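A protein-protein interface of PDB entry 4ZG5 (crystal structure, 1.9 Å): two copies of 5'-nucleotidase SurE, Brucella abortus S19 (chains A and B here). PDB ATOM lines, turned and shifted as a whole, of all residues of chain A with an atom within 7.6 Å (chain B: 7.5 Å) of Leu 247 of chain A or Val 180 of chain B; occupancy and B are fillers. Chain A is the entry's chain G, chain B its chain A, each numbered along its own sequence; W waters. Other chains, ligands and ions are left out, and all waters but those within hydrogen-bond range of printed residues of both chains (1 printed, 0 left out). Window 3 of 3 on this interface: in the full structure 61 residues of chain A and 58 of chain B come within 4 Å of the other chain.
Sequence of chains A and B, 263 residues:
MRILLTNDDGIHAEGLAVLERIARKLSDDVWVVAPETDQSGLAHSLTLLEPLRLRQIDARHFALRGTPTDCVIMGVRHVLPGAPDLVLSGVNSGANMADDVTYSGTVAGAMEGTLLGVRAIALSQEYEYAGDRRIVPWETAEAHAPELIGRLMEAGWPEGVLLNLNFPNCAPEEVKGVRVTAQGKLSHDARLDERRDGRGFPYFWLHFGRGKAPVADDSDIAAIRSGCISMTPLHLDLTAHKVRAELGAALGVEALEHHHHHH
No position is printed for both chains.
Of the 12 pairs that touch across the chains among the printed residues, none has its exchanged pair printed and touching as well.
Of the 13 printed residues of chain A, 7 touch a printed residue of chain B.
Along chain A the printed residues that touch a printed residue of chain B span positions 239 to 252.
Of the 15 printed residues of chain B, 6 touch a printed residue of chain A.
Among the printed residues, 12 pairs touch across the chains.
Among the printed residues, Asp or Glu carboxylates within 4 Å of a Lys or Arg side-chain nitrogen of the other chain: Arg 244 of chain A with Asp 218 of chain B.
C of Ala 182 of chain B touches OG1 of Thr 239 of chain A, 3.9 Å away.
O of Pro 233 of chain B touches CA of Thr 239 of chain A (3.5 Å).
Arg 244 of chain A touches Val 180 of chain B (O to CG1, 3.7 Å).
Ala 182 of chain B touches Arg 244 of chain A (CB to NH1, 3.7 Å).
Arg 244 of chain A touches Pro 233 of chain B (CG to CG, 3.9 Å).
Leu 247 of chain A touches Val 180 of chain B (CB to CG2, 3.4 Å).
CB of Ala 250 of chain A touches O of Val 178 of chain B, 3.8 Å away.
O of Leu 251 of chain A touches CG of Arg 179 of chain B (3.9 Å).
O of Val 180 of chain B touches CA of Gly 252 of chain A, 3.5 Å away.
Water W1 lies within hydrogen-bond range of OD2 of Asp 218 of chain B and NH1 of Arg 244 of chain A.
Of chain B, only Val 180 comes within 4 Å of Leu 247 of chain A.
Of chain A, only Arg 244, Leu 247, Leu 251 and Gly 252 come within 4 Å of Val 180 of chain B.
Printed residues of chain B within 4 Å of Arg 244 of chain A: Val 180 (3.7 Å), Ala 182 (3.7 Å), Asp 218 (3.0 Å) and Pro 233 (3.9 Å).
Printed residues of chain B within 4 Å of Leu 251 of chain A: Arg 179 and Val 180.
Printed residues of chain A within 4 Å of Pro 233 of chain B: Thr 239 (3.5 Å), Ala 240 (2.9 Å) and Arg 244 (3.9 Å).
Ser 230 of chain B touches none of the printed residues of chain A.
The backbone carbonyl oxygen of Leu 251 of chain A lies within hydrogen-bond range of the backbone NH of Val 180 of chain B.
The side-chain carboxylate (OD2) of Asp 218 of chain B lies within salt-bridge range of the guanidinium group (NH2) of Arg 244 of chain A (3.0 Å).
The backbone carbonyl oxygen (O) of Pro 233 of chain B lies within hydrogen-bond range of the backbone NH (N) of Ala 240 of chain A, at 2.9 Å.
The backbone NH of Arg 179 of chain B sits at hydrogen-bond distance from the backbone carbonyl oxygen of Ile 229 of chain B, 2.9 Å away.
The backbone carbonyl oxygen of Arg 179 of chain B is in hydrogen-bond range of the backbone NH of Met 231 of chain B (3.1 Å).
The backbone carbonyl oxygen (O) of Asp 218 of chain B lies within hydrogen-bond range of the backbone NH (N) of Ala 182 of chain B, at 3.0 Å.
The backbone NH (N) of Asp 220 of chain B sits at hydrogen-bond distance from the backbone carbonyl oxygen (O) of Ala 182 of chain B, 2.8 Å away.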
ATOM      1  N   THR A 239     -20.023  17.135 -10.305  1.00  0.00           N
ATOM      2  CA  THR A 239     -19.156  18.242  -9.948  1.00  0.00           C
ATOM      3  C   THR A 239     -19.903  19.150  -8.956  1.00  0.00           C
ATOM      4  O   THR A 239     -21.101  19.463  -9.143  1.00  0.00           O
ATOM      5  CB  THR A 239     -18.752  19.116 -11.175  1.00  0.00           C
ATOM      6  OG1 THR A 239     -18.342  18.258 -12.250  1.00  0.00           O
ATOM      7  CG2 THR A 239     -17.700  20.097 -10.817  1.00  0.00           C
ATOM      8  N   ALA A 240     -19.179  19.569  -7.942  1.00  0.00           N
ATOM      9  CA  ALA A 240     -19.660  20.576  -7.033  1.00  0.00           C
ATOM     10  C   ALA A 240     -19.212  21.919  -7.600  1.00  0.00           C
ATOM     11  O   ALA A 240     -18.263  22.535  -7.156  1.00  0.00           O
ATOM     12  CB  ALA A 240     -19.102  20.332  -5.638  1.00  0.00           C
ATOM     13  N   HIS A 241     -19.984  22.388  -8.576  1.00  0.00           N
ATOM     14  CA  HIS A 241     -19.682  23.580  -9.305  1.00  0.00           C
ATOM     15  C   HIS A 241     -19.536  24.791  -8.458  1.00  0.00           C
ATOM     16  O   HIS A 241     -18.589  25.551  -8.659  1.00  0.00           O
ATOM     17  CB  HIS A 241     -20.739  23.807 -10.383  1.00  0.00           C
ATOM     18  CG  HIS A 241     -20.642  22.831 -11.497  1.00  0.00           C
ATOM     19  ND1 HIS A 241     -21.572  21.833 -11.720  1.00  0.00           N
ATOM     20  CD2 HIS A 241     -19.688  22.685 -12.443  1.00  0.00           C
ATOM     21  CE1 HIS A 241     -21.205  21.123 -12.775  1.00  0.00           C
ATOM     22  NE2 HIS A 241     -20.067  21.640 -13.238  1.00  0.00           N
ATOM     23  N   VAL A 243     -18.334  25.207  -5.751  1.00  0.00           N
ATOM     24  CA  VAL A 243     -17.155  25.122  -4.936  1.00  0.00           C
ATOM     25  C   VAL A 243     -15.876  25.393  -5.711  1.00  0.00           C
ATOM     26  O   VAL A 243     -14.866  25.695  -5.143  1.00  0.00           O
ATOM     27  CB  VAL A 243     -17.110  23.733  -4.288  1.00  0.00           C
ATOM     28  CG1 VAL A 243     -15.826  23.473  -3.688  1.00  0.00           C
ATOM     29  CG2 VAL A 243     -18.173  23.620  -3.273  1.00  0.00           C
ATOM     30  N   ARG A 244     -15.930  25.263  -7.018  1.00  0.00           N
ATOM     31  CA  ARG A 244     -14.757  25.395  -7.831  1.00  0.00           C
ATOM     32  C   ARG A 244     -13.991  26.683  -7.602  1.00  0.00           C
ATOM     33  O   ARG A 244     -12.807  26.665  -7.482  1.00  0.00           O
ATOM     34  CB  ARG A 244     -15.125  25.288  -9.288  1.00  0.00           C
ATOM     35  CG  ARG A 244     -15.352  23.904  -9.760  1.00  0.00           C
ATOM     36  CD  ARG A 244     -16.139  23.897 -11.002  1.00  0.00           C
ATOM     37  NE  ARG A 244     -15.337  24.294 -12.126  1.00  0.00           N
ATOM     38  CZ  ARG A 244     -15.815  24.452 -13.349  1.00  0.00           C
ATOM     39  NH1 ARG A 244     -17.087  24.245 -13.622  1.00  0.00           N
ATOM     40  NH2 ARG A 244     -15.009  24.798 -14.302  1.00  0.00           N
ATOM     41  N   ALA A 245     -14.691  27.804  -7.561  1.00  0.00           N
ATOM     42  CA  ALA A 245     -14.043  29.096  -7.397  1.00  0.00           C
ATOM     43  C   ALA A 245     -13.161  29.168  -6.168  1.00  0.00           C
ATOM     44  O   ALA A 245     -12.082  29.646  -6.260  1.00  0.00           O
ATOM     45  CB  ALA A 245     -15.038  30.179  -7.395  1.00  0.00           C
ATOM     46  N   GLU A 246     -13.541  28.612  -5.043  1.00  0.00           N
ATOM     47  CA  GLU A 246     -12.523  28.469  -4.040  1.00  0.00           C
ATOM     48  C   GLU A 246     -11.538  27.471  -4.597  1.00  0.00           C
ATOM     49  O   GLU A 246     -11.612  26.296  -4.375  1.00  0.00           O
ATOM     50  CB  GLU A 246     -13.044  28.032  -2.703  1.00  0.00           C
ATOM     51  CG  GLU A 246     -14.467  27.678  -2.710  1.00  0.00           C
ATOM     52  CD  GLU A 246     -15.226  28.751  -3.335  1.00  0.00           C
ATOM     53  OE1 GLU A 246     -16.400  28.553  -3.686  1.00  0.00           O
ATOM     54  OE2 GLU A 246     -14.629  29.826  -3.438  1.00  0.00           O
ATOM     55  N   LEU A 247     -10.649  28.014  -5.404  1.00  0.00           N
ATOM     56  CA  LEU A 247      -9.381  27.479  -5.772  1.00  0.00           C
ATOM     57  C   LEU A 247      -8.394  28.570  -5.349  1.00  0.00           C
ATOM     58  O   LEU A 247      -8.273  29.548  -6.033  1.00  0.00           O
ATOM     59  CB  LEU A 247      -9.314  27.402  -7.272  1.00  0.00           C
ATOM     60  N   GLY A 248      -7.724  28.409  -4.206  1.00  0.00           N
ATOM     61  CA  GLY A 248      -6.549  29.191  -3.870  1.00  0.00           C
ATOM     62  C   GLY A 248      -5.403  28.203  -3.893  1.00  0.00           C
ATOM     63  O   GLY A 248      -5.447  27.306  -3.093  1.00  0.00           O
ATOM     64  N   ALA A 249      -4.428  28.292  -4.811  1.00  0.00           N
ATOM     65  CA  ALA A 249      -4.175  29.454  -5.674  1.00  0.00           C
ATOM     66  C   ALA A 249      -3.960  29.190  -7.168  1.00  0.00           C
ATOM     67  O   ALA A 249      -2.896  29.466  -7.694  1.00  0.00           O
ATOM     68  CB  ALA A 249      -2.982  30.199  -5.160  1.00  0.00           C
ATOM     69  N   ALA A 250      -4.968  28.694  -7.863  1.00  0.00           N
ATOM     70  CA  ALA A 250      -4.850  28.464  -9.282  1.00  0.00           C
ATOM     71  C   ALA A 250      -6.136  28.577 -10.039  1.00  0.00           C
ATOM     72  O   ALA A 250      -7.192  28.683  -9.462  1.00  0.00           O
ATOM     73  CB  ALA A 250      -4.227  27.161  -9.544  1.00  0.00           C
ATOM     74  N   LEU A 251      -6.020  28.576 -11.355  1.00  0.00           N
ATOM     75  CA  LEU A 251      -7.196  28.704 -12.247  1.00  0.00           C
ATOM     76  C   LEU A 251      -8.348  27.697 -12.012  1.00  0.00           C
ATOM     77  O   LEU A 251      -8.098  26.555 -11.555  1.00  0.00           O
ATOM     78  CB  LEU A 251      -6.767  28.612 -13.735  1.00  0.00           C
ATOM     79  N   GLY A 252      -9.577  28.159 -12.335  1.00  0.00           N
ATOM     80  CA  GLY A 252     -10.804  27.353 -12.437  1.00  0.00           C
ATOM     81  C   GLY A 252     -11.645  27.342 -11.157  1.00  0.00           C
ATOM     82  O   GLY A 252     -11.268  27.909 -10.133  1.00  0.00           O
ATOM     83  N   LEU B 152      -4.765  21.807   0.399  1.00  0.00           N
ATOM     84  CA  LEU B 152      -6.202  21.570   0.469  1.00  0.00           C
ATOM     85  C   LEU B 152      -6.657  21.409   1.895  1.00  0.00           C
ATOM     86  O   LEU B 152      -7.680  21.895   2.253  1.00  0.00           O
ATOM     87  CB  LEU B 152      -6.554  20.323  -0.291  1.00  0.00           C
ATOM     88  CG  LEU B 152      -6.339  20.437  -1.782  1.00  0.00           C
ATOM     89  CD1 LEU B 152      -6.264  19.087  -2.437  1.00  0.00           C
ATOM     90  CD2 LEU B 152      -7.455  21.287  -2.385  1.00  0.00           C
ATOM     91  N   VAL B 178      -1.614  22.823 -12.270  1.00  0.00           N
ATOM     92  CA  VAL B 178      -2.791  22.183 -11.672  1.00  0.00           C
ATOM     93  C   VAL B 178      -3.981  23.070 -11.974  1.00  0.00           C
ATOM     94  O   VAL B 178      -3.857  24.309 -12.027  1.00  0.00           O
ATOM     95  CB  VAL B 178      -2.663  22.007 -10.145  1.00  0.00           C
ATOM     96  CG1 VAL B 178      -1.357  21.315  -9.807  1.00  0.00           C
ATOM     97  CG2 VAL B 178      -2.628  23.354  -9.437  1.00  0.00           C
ATOM     98  N   ARG B 179      -5.119  22.459 -12.183  1.00  0.00           N
ATOM     99  CA  ARG B 179      -6.291  23.208 -12.533  1.00  0.00           C
ATOM    100  C   ARG B 179      -7.480  22.629 -11.756  1.00  0.00           C
ATOM    101  O   ARG B 179      -7.591  21.449 -11.613  1.00  0.00           O
ATOM    102  CB  ARG B 179      -6.585  23.054 -14.003  1.00  0.00           C
ATOM    103  CG  ARG B 179      -7.136  24.325 -14.597  1.00  0.00           C
ATOM    104  CD  ARG B 179      -7.966  24.206 -15.874  1.00  0.00           C
ATOM    105  NE  ARG B 179      -9.032  25.245 -15.908  1.00  0.00           N
ATOM    106  CZ  ARG B 179      -9.553  25.804 -17.017  1.00  0.00           C
ATOM    107  NH1 ARG B 179      -9.082  25.499 -18.220  1.00  0.00           N
ATOM    108  NH2 ARG B 179     -10.532  26.718 -16.905  1.00  0.00           N
ATOM    109  N   VAL B 180      -8.335  23.487 -11.243  1.00  0.00           N
ATOM    110  CA  VAL B 180      -9.583  23.057 -10.673  1.00  0.00           C
ATOM    111  C   VAL B 180     -10.557  22.876 -11.807  1.00  0.00           C
ATOM    112  O   VAL B 180     -10.873  23.832 -12.550  1.00  0.00           O
ATOM    113  CB  VAL B 180     -10.131  24.075  -9.677  1.00  0.00           C
ATOM    114  CG1 VAL B 180     -11.499  23.602  -9.182  1.00  0.00           C
ATOM    115  CG2 VAL B 180      -9.153  24.217  -8.524  1.00  0.00           C
ATOM    116  N   THR B 181     -10.972  21.650 -12.011  1.00  0.00           N
ATOM    117  CA  THR B 181     -11.711  21.273 -13.193  1.00  0.00           C
ATOM    118  C   THR B 181     -13.142  20.883 -12.859  1.00  0.00           C
ATOM    119  O   THR B 181     -13.480  20.607 -11.720  1.00  0.00           O
ATOM    120  CB  THR B 181     -10.998  20.077 -13.860  1.00  0.00           C
ATOM    121  OG1 THR B 181     -10.855  19.027 -12.913  1.00  0.00           O
ATOM    122  CG2 THR B 181      -9.554  20.514 -14.363  1.00  0.00           C
ATOM    123  N   ALA B 182     -13.922  20.743 -13.920  1.00  0.00           N
ATOM    124  CA  ALA B 182     -15.212  20.100 -13.946  1.00  0.00           C
ATOM    125  C   ALA B 182     -15.128  18.695 -14.503  1.00  0.00           C
ATOM    126  O   ALA B 182     -14.236  18.348 -15.262  1.00  0.00           O
ATOM    127  CB  ALA B 182     -16.146  20.932 -14.868  1.00  0.00           C
ATOM    128  N   ASP B 218     -12.627  23.014 -19.814  1.00  0.00           N
ATOM    129  CA  ASP B 218     -12.474  23.130 -18.378  1.00  0.00           C
ATOM    130  C   ASP B 218     -12.636  21.765 -17.697  1.00  0.00           C
ATOM    131  O   ASP B 218     -12.661  21.680 -16.488  1.00  0.00           O
ATOM    132  CB  ASP B 218     -13.449  24.193 -17.806  1.00  0.00           C
ATOM    133  CG  ASP B 218     -14.926  23.777 -17.925  1.00  0.00           C
ATOM    134  OD1 ASP B 218     -15.234  22.839 -18.694  1.00  0.00           O
ATOM    135  OD2 ASP B 218     -15.754  24.363 -17.221  1.00  0.00           O
ATOM    136  N   SER B 219     -12.657  20.679 -18.471  1.00  0.00           N
ATOM    137  CA  SER B 219     -12.811  19.355 -17.912  1.00  0.00           C
ATOM    138  C   SER B 219     -11.520  18.791 -17.340  1.00  0.00           C
ATOM    139  O   SER B 219     -10.401  19.142 -17.757  1.00  0.00           O
ATOM    140  CB  SER B 219     -13.337  18.387 -18.941  1.00  0.00           C
ATOM    141  OG  SER B 219     -12.436  18.204 -19.987  1.00  0.00           O
ATOM    142  N   ASP B 220     -11.702  17.888 -16.405  1.00  0.00           N
ATOM    143  CA  ASP B 220     -10.625  16.940 -15.970  1.00  0.00           C
ATOM    144  C   ASP B 220      -9.832  16.333 -17.143  1.00  0.00           C
ATOM    145  O   ASP B 220      -8.586  16.442 -17.195  1.00  0.00           O
ATOM    146  CB  ASP B 220     -11.187  15.873 -15.026  1.00  0.00           C
ATOM    147  CG  ASP B 220     -12.459  15.164 -15.557  1.00  0.00           C
ATOM    148  OD1 ASP B 220     -12.866  15.308 -16.733  1.00  0.00           O
ATOM    149  OD2 ASP B 220     -12.985  14.334 -14.760  1.00  0.00           O
ATOM    150  N   ALA B 223      -7.585  18.944 -18.923  1.00  0.00           N
ATOM    151  CA  ALA B 223      -6.452  19.309 -18.115  1.00  0.00           C
ATOM    152  C   ALA B 223      -5.339  18.298 -18.237  1.00  0.00           C
ATOM    153  O   ALA B 223      -4.155  18.638 -18.489  1.00  0.00           O
ATOM    154  CB  ALA B 223      -6.885  19.447 -16.660  1.00  0.00           C
ATOM    155  N   ILE B 229      -2.184  18.644 -13.749  1.00  0.00           N
ATOM    156  CA  ILE B 229      -2.937  17.906 -12.753  1.00  0.00           C
ATOM    157  C   ILE B 229      -4.390  18.418 -12.722  1.00  0.00           C
ATOM    158  O   ILE B 229      -4.604  19.644 -12.712  1.00  0.00           O
ATOM    159  CB  ILE B 229      -2.286  18.088 -11.373  1.00  0.00           C
ATOM    160  CG1 ILE B 229      -0.913  17.385 -11.327  1.00  0.00           C
ATOM    161  CG2 ILE B 229      -3.169  17.552 -10.253  1.00  0.00           C
ATOM    162  CD1 ILE B 229      -0.018  17.856 -10.201  1.00  0.00           C
ATOM    163  N   SER B 230      -5.348  17.488 -12.603  1.00  0.00           N
ATOM    164  CA  SER B 230      -6.747  17.814 -12.467  1.00  0.00           C
ATOM    165  C   SER B 230      -7.280  17.592 -11.064  1.00  0.00           C
ATOM    166  O   SER B 230      -7.071  16.552 -10.461  1.00  0.00           O
ATOM    167  CB  SER B 230      -7.596  17.037 -13.428  1.00  0.00           C
ATOM    168  OG  SER B 230      -8.991  17.174 -13.099  1.00  0.00           O
ATOM    169  N   MET B 231      -7.942  18.607 -10.535  1.00  0.00           N
ATOM    170  CA  MET B 231      -8.593  18.492  -9.241  1.00  0.00           C
ATOM    171  C   MET B 231     -10.037  18.899  -9.399  1.00  0.00           C
ATOM    172  O   MET B 231     -10.335  20.098  -9.640  1.00  0.00           O
ATOM    173  CB  MET B 231      -7.989  19.376  -8.197  1.00  0.00           C
ATOM    174  CG  MET B 231      -8.734  19.249  -6.845  1.00  0.00           C
ATOM    175  SD  MET B 231      -7.893  20.218  -5.592  1.00  0.00           S
ATOM    176  CE  MET B 231      -6.122  20.129  -6.091  1.00  0.00           C
ATOM    177  N   THR B 232     -10.932  17.944  -9.260  1.00  0.00           N
ATOM    178  CA  THR B 232     -12.368  18.196  -9.401  1.00  0.00           C
ATOM    179  C   THR B 232     -13.032  18.002  -8.041  1.00  0.00           C
ATOM    180  O   THR B 232     -12.933  16.929  -7.431  1.00  0.00           O
ATOM    181  CB  THR B 232     -13.037  17.225 -10.350  1.00  0.00           C
ATOM    182  OG1 THR B 232     -12.356  17.226 -11.596  1.00  0.00           O
ATOM    183  CG2 THR B 232     -14.512  17.626 -10.595  1.00  0.00           C
ATOM    184  N   PRO B 233     -13.706  19.039  -7.525  1.00  0.00           N
ATOM    185  CA  PRO B 233     -14.581  18.795  -6.332  1.00  0.00           C
ATOM    186  C   PRO B 233     -15.883  18.119  -6.724  1.00  0.00           C
ATOM    187  O   PRO B 233     -16.500  18.521  -7.734  1.00  0.00           O
ATOM    188  CB  PRO B 233     -14.872  20.200  -5.818  1.00  0.00           C
ATOM    189  CG  PRO B 233     -14.808  21.084  -7.065  1.00  0.00           C
ATOM    190  CD  PRO B 233     -13.896  20.380  -8.092  1.00  0.00           C
HETATM  191  O   HOH W   1     -18.132  24.024 -16.452  1.00  0.00           O
